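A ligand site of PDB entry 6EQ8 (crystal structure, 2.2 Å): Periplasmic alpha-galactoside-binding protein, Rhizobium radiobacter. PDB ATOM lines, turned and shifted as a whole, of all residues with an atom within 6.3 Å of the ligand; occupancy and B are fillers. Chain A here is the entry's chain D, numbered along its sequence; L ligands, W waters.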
ATOM      1  N   GLY A 109       2.674 -29.867   6.598  1.00  0.00           N
ATOM      2  CA  GLY A 109       2.433 -28.444   6.452  1.00  0.00           C
ATOM      3  C   GLY A 109       3.333 -27.524   7.263  1.00  0.00           C
ATOM      4  O   GLY A 109       3.212 -26.313   7.127  1.00  0.00           O
ATOM      5  N   TRP A 110       4.206 -28.088   8.122  1.00  0.00           N
ATOM      6  CA  TRP A 110       5.170 -27.355   8.976  1.00  0.00           C
ATOM      7  C   TRP A 110       4.471 -26.450  10.014  1.00  0.00           C
ATOM      8  O   TRP A 110       3.328 -26.728  10.380  1.00  0.00           O
ATOM      9  CB  TRP A 110       6.201 -26.571   8.118  1.00  0.00           C
ATOM     10  CG  TRP A 110       6.907 -27.430   7.100  1.00  0.00           C
ATOM     11  CD1 TRP A 110       6.679 -27.462   5.751  1.00  0.00           C
ATOM     12  CD2 TRP A 110       7.902 -28.428   7.368  1.00  0.00           C
ATOM     13  NE1 TRP A 110       7.500 -28.397   5.155  1.00  0.00           N
ATOM     14  CE2 TRP A 110       8.255 -29.017   6.128  1.00  0.00           C
ATOM     15  CE3 TRP A 110       8.544 -28.878   8.539  1.00  0.00           C
ATOM     16  CZ2 TRP A 110       9.238 -30.016   6.024  1.00  0.00           C
ATOM     17  CZ3 TRP A 110       9.499 -29.876   8.435  1.00  0.00           C
ATOM     18  CH2 TRP A 110       9.839 -30.422   7.190  1.00  0.00           C
ATOM     19  N   GLY A 111       5.179 -25.411  10.490  1.00  0.00           N
ATOM     20  CA  GLY A 111       4.651 -24.491  11.493  1.00  0.00           C
ATOM     21  C   GLY A 111       4.152 -25.118  12.786  1.00  0.00           C
ATOM     22  O   GLY A 111       3.226 -24.581  13.419  1.00  0.00           O
ATOM     23  N   GLY A 112       4.764 -26.250  13.177  1.00  0.00           N
ATOM     24  CA  GLY A 112       4.462 -26.960  14.412  1.00  0.00           C
ATOM     25  C   GLY A 112       3.632 -28.234  14.318  1.00  0.00           C
ATOM     26  O   GLY A 112       3.618 -28.989  15.291  1.00  0.00           O
ATOM     27  N   ILE A 113       2.924 -28.477  13.207  1.00  0.00           N
ATOM     28  CA  ILE A 113       2.055 -29.662  13.047  1.00  0.00           C
ATOM     29  C   ILE A 113       2.850 -30.999  13.247  1.00  0.00           C
ATOM     30  O   ILE A 113       2.463 -31.773  14.122  1.00  0.00           O
ATOM     31  CB  ILE A 113       1.212 -29.638  11.742  1.00  0.00           C
ATOM     32  CG1 ILE A 113       0.227 -30.837  11.691  1.00  0.00           C
ATOM     33  CG2 ILE A 113       2.068 -29.557  10.494  1.00  0.00           C
ATOM     34  CD1 ILE A 113      -1.088 -30.580  11.120  1.00  0.00           C
ATOM     35  N   ASP A 114       3.931 -31.238  12.474  1.00  0.00           N
ATOM     36  CA  ASP A 114       4.709 -32.478  12.617  1.00  0.00           C
ATOM     37  C   ASP A 114       5.502 -32.512  13.925  1.00  0.00           C
ATOM     38  O   ASP A 114       5.751 -33.597  14.453  1.00  0.00           O
ATOM     39  CB  ASP A 114       5.602 -32.735  11.396  1.00  0.00           C
ATOM     40  CG  ASP A 114       6.640 -31.669  11.147  1.00  0.00           C
ATOM     41  OD1 ASP A 114       6.261 -30.546  10.770  1.00  0.00           O
ATOM     42  OD2 ASP A 114       7.815 -31.968  11.317  1.00  0.00           O
ATOM     43  N   ILE A 115       5.880 -31.332  14.447  1.00  0.00           N
ATOM     44  CA  ILE A 115       6.529 -31.217  15.750  1.00  0.00           C
ATOM     45  C   ILE A 115       5.563 -31.783  16.846  1.00  0.00           C
ATOM     46  O   ILE A 115       5.983 -32.577  17.685  1.00  0.00           O
ATOM     47  CB  ILE A 115       6.965 -29.750  16.024  1.00  0.00           C
ATOM     48  CG1 ILE A 115       8.243 -29.392  15.194  1.00  0.00           C
ATOM     49  CG2 ILE A 115       7.140 -29.478  17.532  1.00  0.00           C
ATOM     50  CD1 ILE A 115       8.736 -27.880  15.240  1.00  0.00           C
ATOM     51  N   GLY A 192      12.771 -34.142   7.181  1.00  0.00           N
ATOM     52  CA  GLY A 192      13.865 -33.352   7.711  1.00  0.00           C
ATOM     53  C   GLY A 192      15.156 -33.469   6.924  1.00  0.00           C
ATOM     54  O   GLY A 192      16.043 -32.615   7.047  1.00  0.00           O
ATOM     55  N   TYR A 232      14.118 -34.563  17.585  1.00  0.00           N
ATOM     56  CA  TYR A 232      13.499 -34.098  16.353  1.00  0.00           C
ATOM     57  C   TYR A 232      14.541 -33.460  15.416  1.00  0.00           C
ATOM     58  O   TYR A 232      15.388 -32.703  15.893  1.00  0.00           O
ATOM     59  CB  TYR A 232      12.340 -33.129  16.677  1.00  0.00           C
ATOM     60  CG  TYR A 232      11.683 -32.494  15.470  1.00  0.00           C
ATOM     61  CD1 TYR A 232      12.223 -31.351  14.874  1.00  0.00           C
ATOM     62  CD2 TYR A 232      10.520 -33.026  14.907  1.00  0.00           C
ATOM     63  CE1 TYR A 232      11.648 -30.778  13.742  1.00  0.00           C
ATOM     64  CE2 TYR A 232       9.917 -32.437  13.793  1.00  0.00           C
ATOM     65  CZ  TYR A 232      10.469 -31.304  13.238  1.00  0.00           C
ATOM     66  OH  TYR A 232       9.879 -30.693  12.159  1.00  0.00           O
ATOM     67  N   TRP A 317       3.109 -17.774   5.190  1.00  0.00           N
ATOM     68  CA  TRP A 317       4.001 -17.497   6.315  1.00  0.00           C
ATOM     69  C   TRP A 317       3.851 -16.047   6.799  1.00  0.00           C
ATOM     70  O   TRP A 317       3.870 -15.820   8.006  1.00  0.00           O
ATOM     71  CB  TRP A 317       5.447 -17.901   6.009  1.00  0.00           C
ATOM     72  CG  TRP A 317       5.611 -19.376   5.790  1.00  0.00           C
ATOM     73  CD1 TRP A 317       5.912 -20.001   4.619  1.00  0.00           C
ATOM     74  CD2 TRP A 317       5.362 -20.423   6.755  1.00  0.00           C
ATOM     75  NE1 TRP A 317       5.913 -21.365   4.800  1.00  0.00           N
ATOM     76  CE2 TRP A 317       5.581 -21.656   6.095  1.00  0.00           C
ATOM     77  CE3 TRP A 317       4.994 -20.450   8.113  1.00  0.00           C
ATOM     78  CZ2 TRP A 317       5.419 -22.893   6.739  1.00  0.00           C
ATOM     79  CZ3 TRP A 317       4.811 -21.681   8.737  1.00  0.00           C
ATOM     80  CH2 TRP A 317       5.046 -22.879   8.056  1.00  0.00           C
ATOM     81  N   ARG A 320       0.743 -15.611   9.024  1.00  0.00           N
ATOM     82  CA  ARG A 320       0.941 -16.069  10.397  1.00  0.00           C
ATOM     83  C   ARG A 320       1.310 -14.869  11.302  1.00  0.00           C
ATOM     84  O   ARG A 320       0.796 -14.773  12.423  1.00  0.00           O
ATOM     85  CB  ARG A 320       1.993 -17.197  10.475  1.00  0.00           C
ATOM     86  CG  ARG A 320       2.188 -17.694  11.926  1.00  0.00           C
ATOM     87  CD  ARG A 320       3.225 -18.758  12.121  1.00  0.00           C
ATOM     88  NE  ARG A 320       4.545 -18.328  11.666  1.00  0.00           N
ATOM     89  CZ  ARG A 320       5.625 -19.102  11.643  1.00  0.00           C
ATOM     90  NH1 ARG A 320       5.560 -20.351  12.076  1.00  0.00           N
ATOM     91  NH2 ARG A 320       6.770 -18.621  11.203  1.00  0.00           N
ATOM     92  N   PHE A 331       0.093 -17.844  17.793  1.00  0.00           N
ATOM     93  CA  PHE A 331       1.525 -18.023  17.746  1.00  0.00           C
ATOM     94  C   PHE A 331       2.111 -17.605  16.411  1.00  0.00           C
ATOM     95  O   PHE A 331       1.515 -17.827  15.368  1.00  0.00           O
ATOM     96  CB  PHE A 331       1.832 -19.527  18.005  1.00  0.00           C
ATOM     97  CG  PHE A 331       3.299 -19.909  17.982  1.00  0.00           C
ATOM     98  CD1 PHE A 331       3.984 -20.052  16.782  1.00  0.00           C
ATOM     99  CD2 PHE A 331       3.983 -20.158  19.168  1.00  0.00           C
ATOM    100  CE1 PHE A 331       5.348 -20.352  16.769  1.00  0.00           C
ATOM    101  CE2 PHE A 331       5.322 -20.549  19.153  1.00  0.00           C
ATOM    102  CZ  PHE A 331       6.002 -20.628  17.947  1.00  0.00           C
ATOM    103  N   ASN A 333       6.452 -17.146  14.652  1.00  0.00           N
ATOM    104  CA  ASN A 333       7.901 -16.994  14.636  1.00  0.00           C
ATOM    105  C   ASN A 333       8.111 -15.881  13.613  1.00  0.00           C
ATOM    106  O   ASN A 333       7.909 -16.095  12.416  1.00  0.00           O
ATOM    107  CB  ASN A 333       8.628 -18.290  14.217  1.00  0.00           C
ATOM    108  CG  ASN A 333       8.594 -19.407  15.238  1.00  0.00           C
ATOM    109  OD1 ASN A 333       8.676 -19.193  16.452  1.00  0.00           O
ATOM    110  ND2 ASN A 333       8.540 -20.627  14.761  1.00  0.00           N
ATOM    111  N   GLU A 335      10.244 -14.089  11.604  1.00  0.00           N
ATOM    112  CA  GLU A 335      11.527 -14.472  11.021  1.00  0.00           C
ATOM    113  C   GLU A 335      11.837 -13.863   9.651  1.00  0.00           C
ATOM    114  O   GLU A 335      12.868 -14.193   9.044  1.00  0.00           O
ATOM    115  CB  GLU A 335      11.510 -15.999  10.907  1.00  0.00           C
ATOM    116  CG  GLU A 335      10.283 -16.465  10.168  1.00  0.00           C
ATOM    117  CD  GLU A 335      10.045 -17.959  10.149  1.00  0.00           C
ATOM    118  OE1 GLU A 335      10.487 -18.673  11.074  1.00  0.00           O
ATOM    119  OE2 GLU A 335       9.412 -18.414   9.178  1.00  0.00           O
ATOM    120  N   ASN A 484      13.043 -21.390  -2.253  1.00  0.00           N
ATOM    121  CA  ASN A 484      11.732 -21.683  -1.684  1.00  0.00           C
ATOM    122  C   ASN A 484      10.873 -20.442  -1.990  1.00  0.00           C
ATOM    123  O   ASN A 484      11.179 -19.330  -1.517  1.00  0.00           O
ATOM    124  CB  ASN A 484      11.821 -21.860  -0.144  1.00  0.00           C
ATOM    125  CG  ASN A 484      10.549 -22.316   0.583  1.00  0.00           C
ATOM    126  OD1 ASN A 484       9.430 -22.340   0.044  1.00  0.00           O
ATOM    127  ND2 ASN A 484      10.703 -22.695   1.850  1.00  0.00           N
ATOM    128  N   TYR A 487       8.550 -17.686   0.942  1.00  0.00           N
ATOM    129  CA  TYR A 487       9.059 -16.572   1.758  1.00  0.00           C
ATOM    130  C   TYR A 487       9.556 -15.416   0.952  1.00  0.00           C
ATOM    131  O   TYR A 487      10.268 -15.617  -0.021  1.00  0.00           O
ATOM    132  CB  TYR A 487      10.217 -17.041   2.665  1.00  0.00           C
ATOM    133  CG  TYR A 487       9.839 -18.177   3.589  1.00  0.00           C
ATOM    134  CD1 TYR A 487       9.844 -19.499   3.140  1.00  0.00           C
ATOM    135  CD2 TYR A 487       9.522 -17.943   4.926  1.00  0.00           C
ATOM    136  CE1 TYR A 487       9.464 -20.541   3.978  1.00  0.00           C
ATOM    137  CE2 TYR A 487       9.212 -18.981   5.782  1.00  0.00           C
ATOM    138  CZ  TYR A 487       9.176 -20.275   5.309  1.00  0.00           C
ATOM    139  OH  TYR A 487       8.832 -21.298   6.146  1.00  0.00           O
ATOM    140  N   SER A 515       8.056 -25.688  -1.278  1.00  0.00           N
ATOM    141  CA  SER A 515       8.791 -26.431  -0.263  1.00  0.00           C
ATOM    142  C   SER A 515       9.064 -27.916  -0.576  1.00  0.00           C
ATOM    143  O   SER A 515      10.223 -28.334  -0.509  1.00  0.00           O
ATOM    144  CB  SER A 515       8.109 -26.298   1.102  1.00  0.00           C
ATOM    145  OG  SER A 515       8.790 -27.000   2.125  1.00  0.00           O
ATOM    146  N   ASN A 516       8.029 -28.695  -0.948  1.00  0.00           N
ATOM    147  CA  ASN A 516       8.190 -30.122  -1.236  1.00  0.00           C
ATOM    148  C   ASN A 516       8.999 -30.389  -2.492  1.00  0.00           C
ATOM    149  O   ASN A 516       9.863 -31.260  -2.473  1.00  0.00           O
ATOM    150  CB  ASN A 516       6.843 -30.860  -1.237  1.00  0.00           C
ATOM    151  CG  ASN A 516       5.856 -30.507  -2.313  1.00  0.00           C
ATOM    152  OD1 ASN A 516       5.562 -31.334  -3.189  1.00  0.00           O
ATOM    153  ND2 ASN A 516       5.152 -29.396  -2.194  1.00  0.00           N
ATOM    154  N   ARG A 518      11.201 -28.222  -3.728  1.00  0.00           N
ATOM    155  CA  ARG A 518      12.526 -27.684  -3.376  1.00  0.00           C
ATOM    156  C   ARG A 518      13.372 -28.742  -2.639  1.00  0.00           C
ATOM    157  O   ARG A 518      14.535 -28.954  -2.987  1.00  0.00           O
ATOM    158  CB  ARG A 518      12.377 -26.382  -2.579  1.00  0.00           C
ATOM    159  CG  ARG A 518      13.686 -25.588  -2.427  1.00  0.00           C
ATOM    160  CD  ARG A 518      13.985 -25.252  -0.979  1.00  0.00           C
ATOM    161  NE  ARG A 518      14.252 -26.442  -0.156  1.00  0.00           N
ATOM    162  CZ  ARG A 518      15.461 -26.937   0.098  1.00  0.00           C
ATOM    163  NH1 ARG A 518      16.539 -26.381  -0.428  1.00  0.00           N
ATOM    164  NH2 ARG A 518      15.605 -28.014   0.857  1.00  0.00           N
ATOM    165  N   ASP A 519      12.758 -29.445  -1.652  1.00  0.00           N
ATOM    166  CA  ASP A 519      13.383 -30.528  -0.878  1.00  0.00           C
ATOM    167  C   ASP A 519      13.815 -31.683  -1.753  1.00  0.00           C
ATOM    168  O   ASP A 519      14.935 -32.172  -1.595  1.00  0.00           O
ATOM    169  CB  ASP A 519      12.426 -31.024   0.228  1.00  0.00           C
ATOM    170  CG  ASP A 519      12.351 -30.155   1.474  1.00  0.00           C
ATOM    171  OD1 ASP A 519      13.211 -29.256   1.623  1.00  0.00           O
ATOM    172  OD2 ASP A 519      11.438 -30.387   2.297  1.00  0.00           O
ATOM    173  N   TYR A 523      17.754 -32.561  -1.895  1.00  0.00           N
ATOM    174  CA  TYR A 523      18.173 -33.883  -1.383  1.00  0.00           C
ATOM    175  C   TYR A 523      18.540 -34.837  -2.524  1.00  0.00           C
ATOM    176  O   TYR A 523      19.429 -35.675  -2.351  1.00  0.00           O
ATOM    177  CB  TYR A 523      17.124 -34.487  -0.416  1.00  0.00           C
ATOM    178  CG  TYR A 523      16.672 -33.557   0.702  1.00  0.00           C
ATOM    179  CD1 TYR A 523      17.498 -32.543   1.183  1.00  0.00           C
ATOM    180  CD2 TYR A 523      15.420 -33.725   1.303  1.00  0.00           C
ATOM    181  CE1 TYR A 523      17.075 -31.680   2.197  1.00  0.00           C
ATOM    182  CE2 TYR A 523      14.996 -32.876   2.329  1.00  0.00           C
ATOM    183  CZ  TYR A 523      15.823 -31.861   2.766  1.00  0.00           C
ATOM    184  OH  TYR A 523      15.399 -31.031   3.787  1.00  0.00           O
ATOM    185  N   ARG A 533      17.814 -21.101   4.426  1.00  0.00           N
ATOM    186  CA  ARG A 533      17.792 -20.670   5.814  1.00  0.00           C
ATOM    187  C   ARG A 533      18.464 -21.799   6.601  1.00  0.00           C
ATOM    188  O   ARG A 533      18.193 -22.972   6.332  1.00  0.00           O
ATOM    189  CB  ARG A 533      16.356 -20.458   6.314  1.00  0.00           C
ATOM    190  CG  ARG A 533      16.275 -19.711   7.632  1.00  0.00           C
ATOM    191  CD  ARG A 533      14.871 -19.321   7.950  1.00  0.00           C
ATOM    192  NE  ARG A 533      13.994 -20.477   8.132  1.00  0.00           N
ATOM    193  CZ  ARG A 533      12.665 -20.419   8.159  1.00  0.00           C
ATOM    194  NH1 ARG A 533      12.048 -19.260   7.994  1.00  0.00           N
ATOM    195  NH2 ARG A 533      11.954 -21.514   8.325  1.00  0.00           N
ATOM    196  N   ILE A 634      13.028 -18.260  18.984  1.00  0.00           N
ATOM    197  CA  ILE A 634      12.238 -18.839  17.904  1.00  0.00           C
ATOM    198  C   ILE A 634      12.914 -20.080  17.352  1.00  0.00           C
ATOM    199  O   ILE A 634      12.232 -20.975  16.875  1.00  0.00           O
ATOM    200  CB  ILE A 634      11.803 -17.849  16.778  1.00  0.00           C
ATOM    201  CG1 ILE A 634      12.989 -17.274  15.954  1.00  0.00           C
ATOM    202  CG2 ILE A 634      10.925 -16.748  17.333  1.00  0.00           C
ATOM    203  CD1 ILE A 634      12.552 -16.850  14.492  1.00  0.00           C
ATOM    204  N   PHE A 635      14.255 -20.132  17.428  1.00  0.00           N
ATOM    205  CA  PHE A 635      15.034 -21.227  16.856  1.00  0.00           C
ATOM    206  C   PHE A 635      16.420 -21.393  17.510  1.00  0.00           C
ATOM    207  O   PHE A 635      17.265 -20.511  17.399  1.00  0.00           O
ATOM    208  CB  PHE A 635      15.180 -21.007  15.327  1.00  0.00           C
ATOM    209  CG  PHE A 635      15.764 -22.162  14.559  1.00  0.00           C
ATOM    210  CD1 PHE A 635      15.077 -23.366  14.458  1.00  0.00           C
ATOM    211  CD2 PHE A 635      16.968 -22.031  13.867  1.00  0.00           C
ATOM    212  CE1 PHE A 635      15.594 -24.431  13.711  1.00  0.00           C
ATOM    213  CE2 PHE A 635      17.491 -23.098  13.126  1.00  0.00           C
ATOM    214  CZ  PHE A 635      16.791 -24.270  13.018  1.00  0.00           C
ATOM    215  N   ASN A 638      15.576 -26.346  18.375  1.00  0.00           N
ATOM    216  CA  ASN A 638      14.454 -26.526  17.470  1.00  0.00           C
ATOM    217  C   ASN A 638      13.647 -25.221  17.444  1.00  0.00           C
ATOM    218  O   ASN A 638      13.992 -24.258  18.137  1.00  0.00           O
ATOM    219  CB  ASN A 638      13.556 -27.726  17.873  1.00  0.00           C
ATOM    220  CG  ASN A 638      12.684 -28.250  16.746  1.00  0.00           C
ATOM    221  OD1 ASN A 638      12.832 -27.873  15.583  1.00  0.00           O
ATOM    222  ND2 ASN A 638      11.756 -29.133  17.080  1.00  0.00           N
ATOM    223  N   TRP A 639      12.571 -25.194  16.649  1.00  0.00           N
ATOM    224  CA  TRP A 639      11.624 -24.106  16.557  1.00  0.00           C
ATOM    225  C   TRP A 639      10.880 -23.946  17.905  1.00  0.00           C
ATOM    226  O   TRP A 639      10.738 -24.929  18.642  1.00  0.00           O
ATOM    227  CB  TRP A 639      10.648 -24.354  15.407  1.00  0.00           C
ATOM    228  CG  TRP A 639      11.329 -24.258  14.077  1.00  0.00           C
ATOM    229  CD1 TRP A 639      11.734 -25.300  13.287  1.00  0.00           C
ATOM    230  CD2 TRP A 639      11.808 -23.062  13.440  1.00  0.00           C
ATOM    231  NE1 TRP A 639      12.401 -24.815  12.176  1.00  0.00           N
ATOM    232  CE2 TRP A 639      12.450 -23.453  12.243  1.00  0.00           C
ATOM    233  CE3 TRP A 639      11.745 -21.687  13.762  1.00  0.00           C
ATOM    234  CZ2 TRP A 639      13.033 -22.518  11.364  1.00  0.00           C
ATOM    235  CZ3 TRP A 639      12.327 -20.766  12.893  1.00  0.00           C
ATOM    236  CH2 TRP A 639      12.967 -21.189  11.703  1.00  0.00           C
ATOM    237  N   GLU A 641       7.809 -23.745  18.697  1.00  0.00           N
ATOM    238  CA  GLU A 641       6.610 -24.587  18.850  1.00  0.00           C
ATOM    239  C   GLU A 641       6.896 -25.792  19.736  1.00  0.00           C
ATOM    240  O   GLU A 641       6.034 -26.239  20.508  1.00  0.00           O
ATOM    241  CB  GLU A 641       6.064 -25.081  17.486  1.00  0.00           C
ATOM    242  CG  GLU A 641       5.462 -23.996  16.619  1.00  0.00           C
ATOM    243  CD  GLU A 641       6.407 -23.367  15.603  1.00  0.00           C
ATOM    244  OE1 GLU A 641       7.607 -23.197  15.918  1.00  0.00           O
ATOM    245  OE2 GLU A 641       5.910 -22.947  14.538  1.00  0.00           O
HETATM  246  C1  LIG L   1       8.581 -22.881  12.036  1.00  0.00           C
HETATM  247  C2  LIG L   1       8.723 -24.261  11.395  1.00  0.00           C
HETATM  248  C3  LIG L   1       8.302 -25.405  12.316  1.00  0.00           C
HETATM  249  C4  LIG L   1      11.325 -26.739   7.061  1.00  0.00           C
HETATM  250  C5  LIG L   1       9.745 -24.829   7.835  1.00  0.00           C
HETATM  251  C6  LIG L   1       9.534 -24.461   6.323  1.00  0.00           C
HETATM  252  C7  LIG L   1       9.702 -25.696   5.427  1.00  0.00           C
HETATM  253  C8  LIG L   1      11.107 -26.327   5.581  1.00  0.00           C
HETATM  254  C9  LIG L   1      11.141 -25.500   8.030  1.00  0.00           C
HETATM  255  C10 LIG L   1       9.120 -21.848  11.055  1.00  0.00           C
HETATM  256  C11 LIG L   1       8.393 -23.342   9.125  1.00  0.00           C
HETATM  257  C12 LIG L   1       8.339 -21.918   9.707  1.00  0.00           C
HETATM  258  O1  LIG L   1       9.700 -23.621   8.620  1.00  0.00           O
HETATM  259  O2  LIG L   1       8.810 -20.970   8.783  1.00  0.00           O
HETATM  260  O3  LIG L   1       8.903 -20.601  11.661  1.00  0.00           O
HETATM  261  O4  LIG L   1       7.197 -22.583  12.267  1.00  0.00           O
HETATM  262  O5  LIG L   1       7.997 -24.314  10.140  1.00  0.00           O
HETATM  263  O6  LIG L   1       8.369 -26.607  11.541  1.00  0.00           O
HETATM  264  O7  LIG L   1      10.427 -23.394   5.917  1.00  0.00           O
HETATM  265  O8  LIG L   1       9.472 -25.310   4.094  1.00  0.00           O
HETATM  266  O9  LIG L   1      11.177 -27.476   4.762  1.00  0.00           O
HETATM  267  O10 LIG L   1      12.627 -27.309   7.190  1.00  0.00           O
HETATM  268  O11 LIG L   1      11.336 -25.843   9.395  1.00  0.00           O
HETATM  269  O   HOH W   1      13.503 -29.876   7.105  1.00  0.00           O
HETATM  270  O   HOH W   2       6.444 -28.306  12.195  1.00  0.00           O
HETATM  271  O   HOH W   3       6.928 -24.386   3.704  1.00  0.00           O
HETATM  272  O   HOH W   4      10.652 -28.056  11.501  1.00  0.00           O
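Trp 110 touches the ligand (CZ2 to O9, 3.4 Å). N of Gly 112 touches C3 of the ligand, at 3.7 Å. Ile 115 touches the ligand (CD1 to C3, 3.9 Å). Trp 317 touches the ligand (CH2 to C11, 3.5 Å). ND2 of Asn 484 touches O8 of the ligand, 3.7 Å away. OD2 of Asp 519 touches O9 of the ligand (3.8 Å). Hydrophobic or aromatic side chains that line the ligand: Trp 110, Ile 115, Trp 317, Tyr 487 and Trp 639. Of the 27 residues printed, 15 come within 4 Å of the ligand.
Water W2 lies within hydrogen-bond range of an oxygen (O6) of the ligand, the side-chain carboxylate of Asp 114 and the backbone NH of Gly 112. Water W4 lies within hydrogen-bond range of an oxygen (O6) of the ligand (2.7 Å) and the side-chain hydroxyl of Tyr 232 (2.8 Å). Water W3 bridges O8 of the ligand (2.7 Å) and NE1 of Trp 317 (3.4 Å).
The side-chain carboxylate (OE2) of Glu 335 is in salt-bridge range of the guanidinium group (NH2) of Arg 320, 3.3 Å away. OE2 of Glu 335 lies within salt-bridge range of NH1 of Arg 533 (3.0 Å). The guanidinium group (NH1) of Arg 320 is in salt-bridge range of the side-chain carboxylate (OE2) of Glu 641. The side-chain carboxylate of Glu 641 is in hydrogen-bond range of the side-chain amide nitrogen of Asn 333, 3.0 Å away. OH of Tyr 487 is in hydrogen-bond range of NE1 of Trp 317 (3.2 Å). O of Asn 333 lies within hydrogen-bond range of NH2 of Arg 320 (3.0 Å). The guanidinium group of Arg 518 is in salt-bridge range of the side-chain carboxylate of Asp 519, at 2.8 Å.
The side-chain carboxylate (OE1) of Glu 335 sits at hydrogen-bond distance from an oxygen (O3) of the ligand, at 2.6 Å. The side-chain carboxylate (OE2) of Glu 641 lies within hydrogen-bond range of an oxygen (O4) of the ligand (2.6 Å). An oxygen (O7) of the ligand is in hydrogen-bond range of the side-chain hydroxyl (OH) of Tyr 487, at 2.6 Å. The side-chain hydroxyl (OG) of Ser 515 sits at hydrogen-bond distance from an oxygen (O8) of the ligand (2.7 Å). NH1 of Arg 320 sits at hydrogen-bond distance from O4 of the ligand. The backbone NH (N) of Gly 111 lies within hydrogen-bond range of an oxygen (O5) of the ligand, at 3.0 Å. An oxygen (O1) of the ligand sits at hydrogen-bond distance from the guanidinium group (NH2) of Arg 533 (3.1 Å). The side-chain amide nitrogen (ND2) of Asn 333 sits at hydrogen-bond distance from an oxygen (O3) of the ligand, 3.1 Å away. NE1 of Trp 639 lies within hydrogen-bond range of O11 of the ligand, at 3.2 Å.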
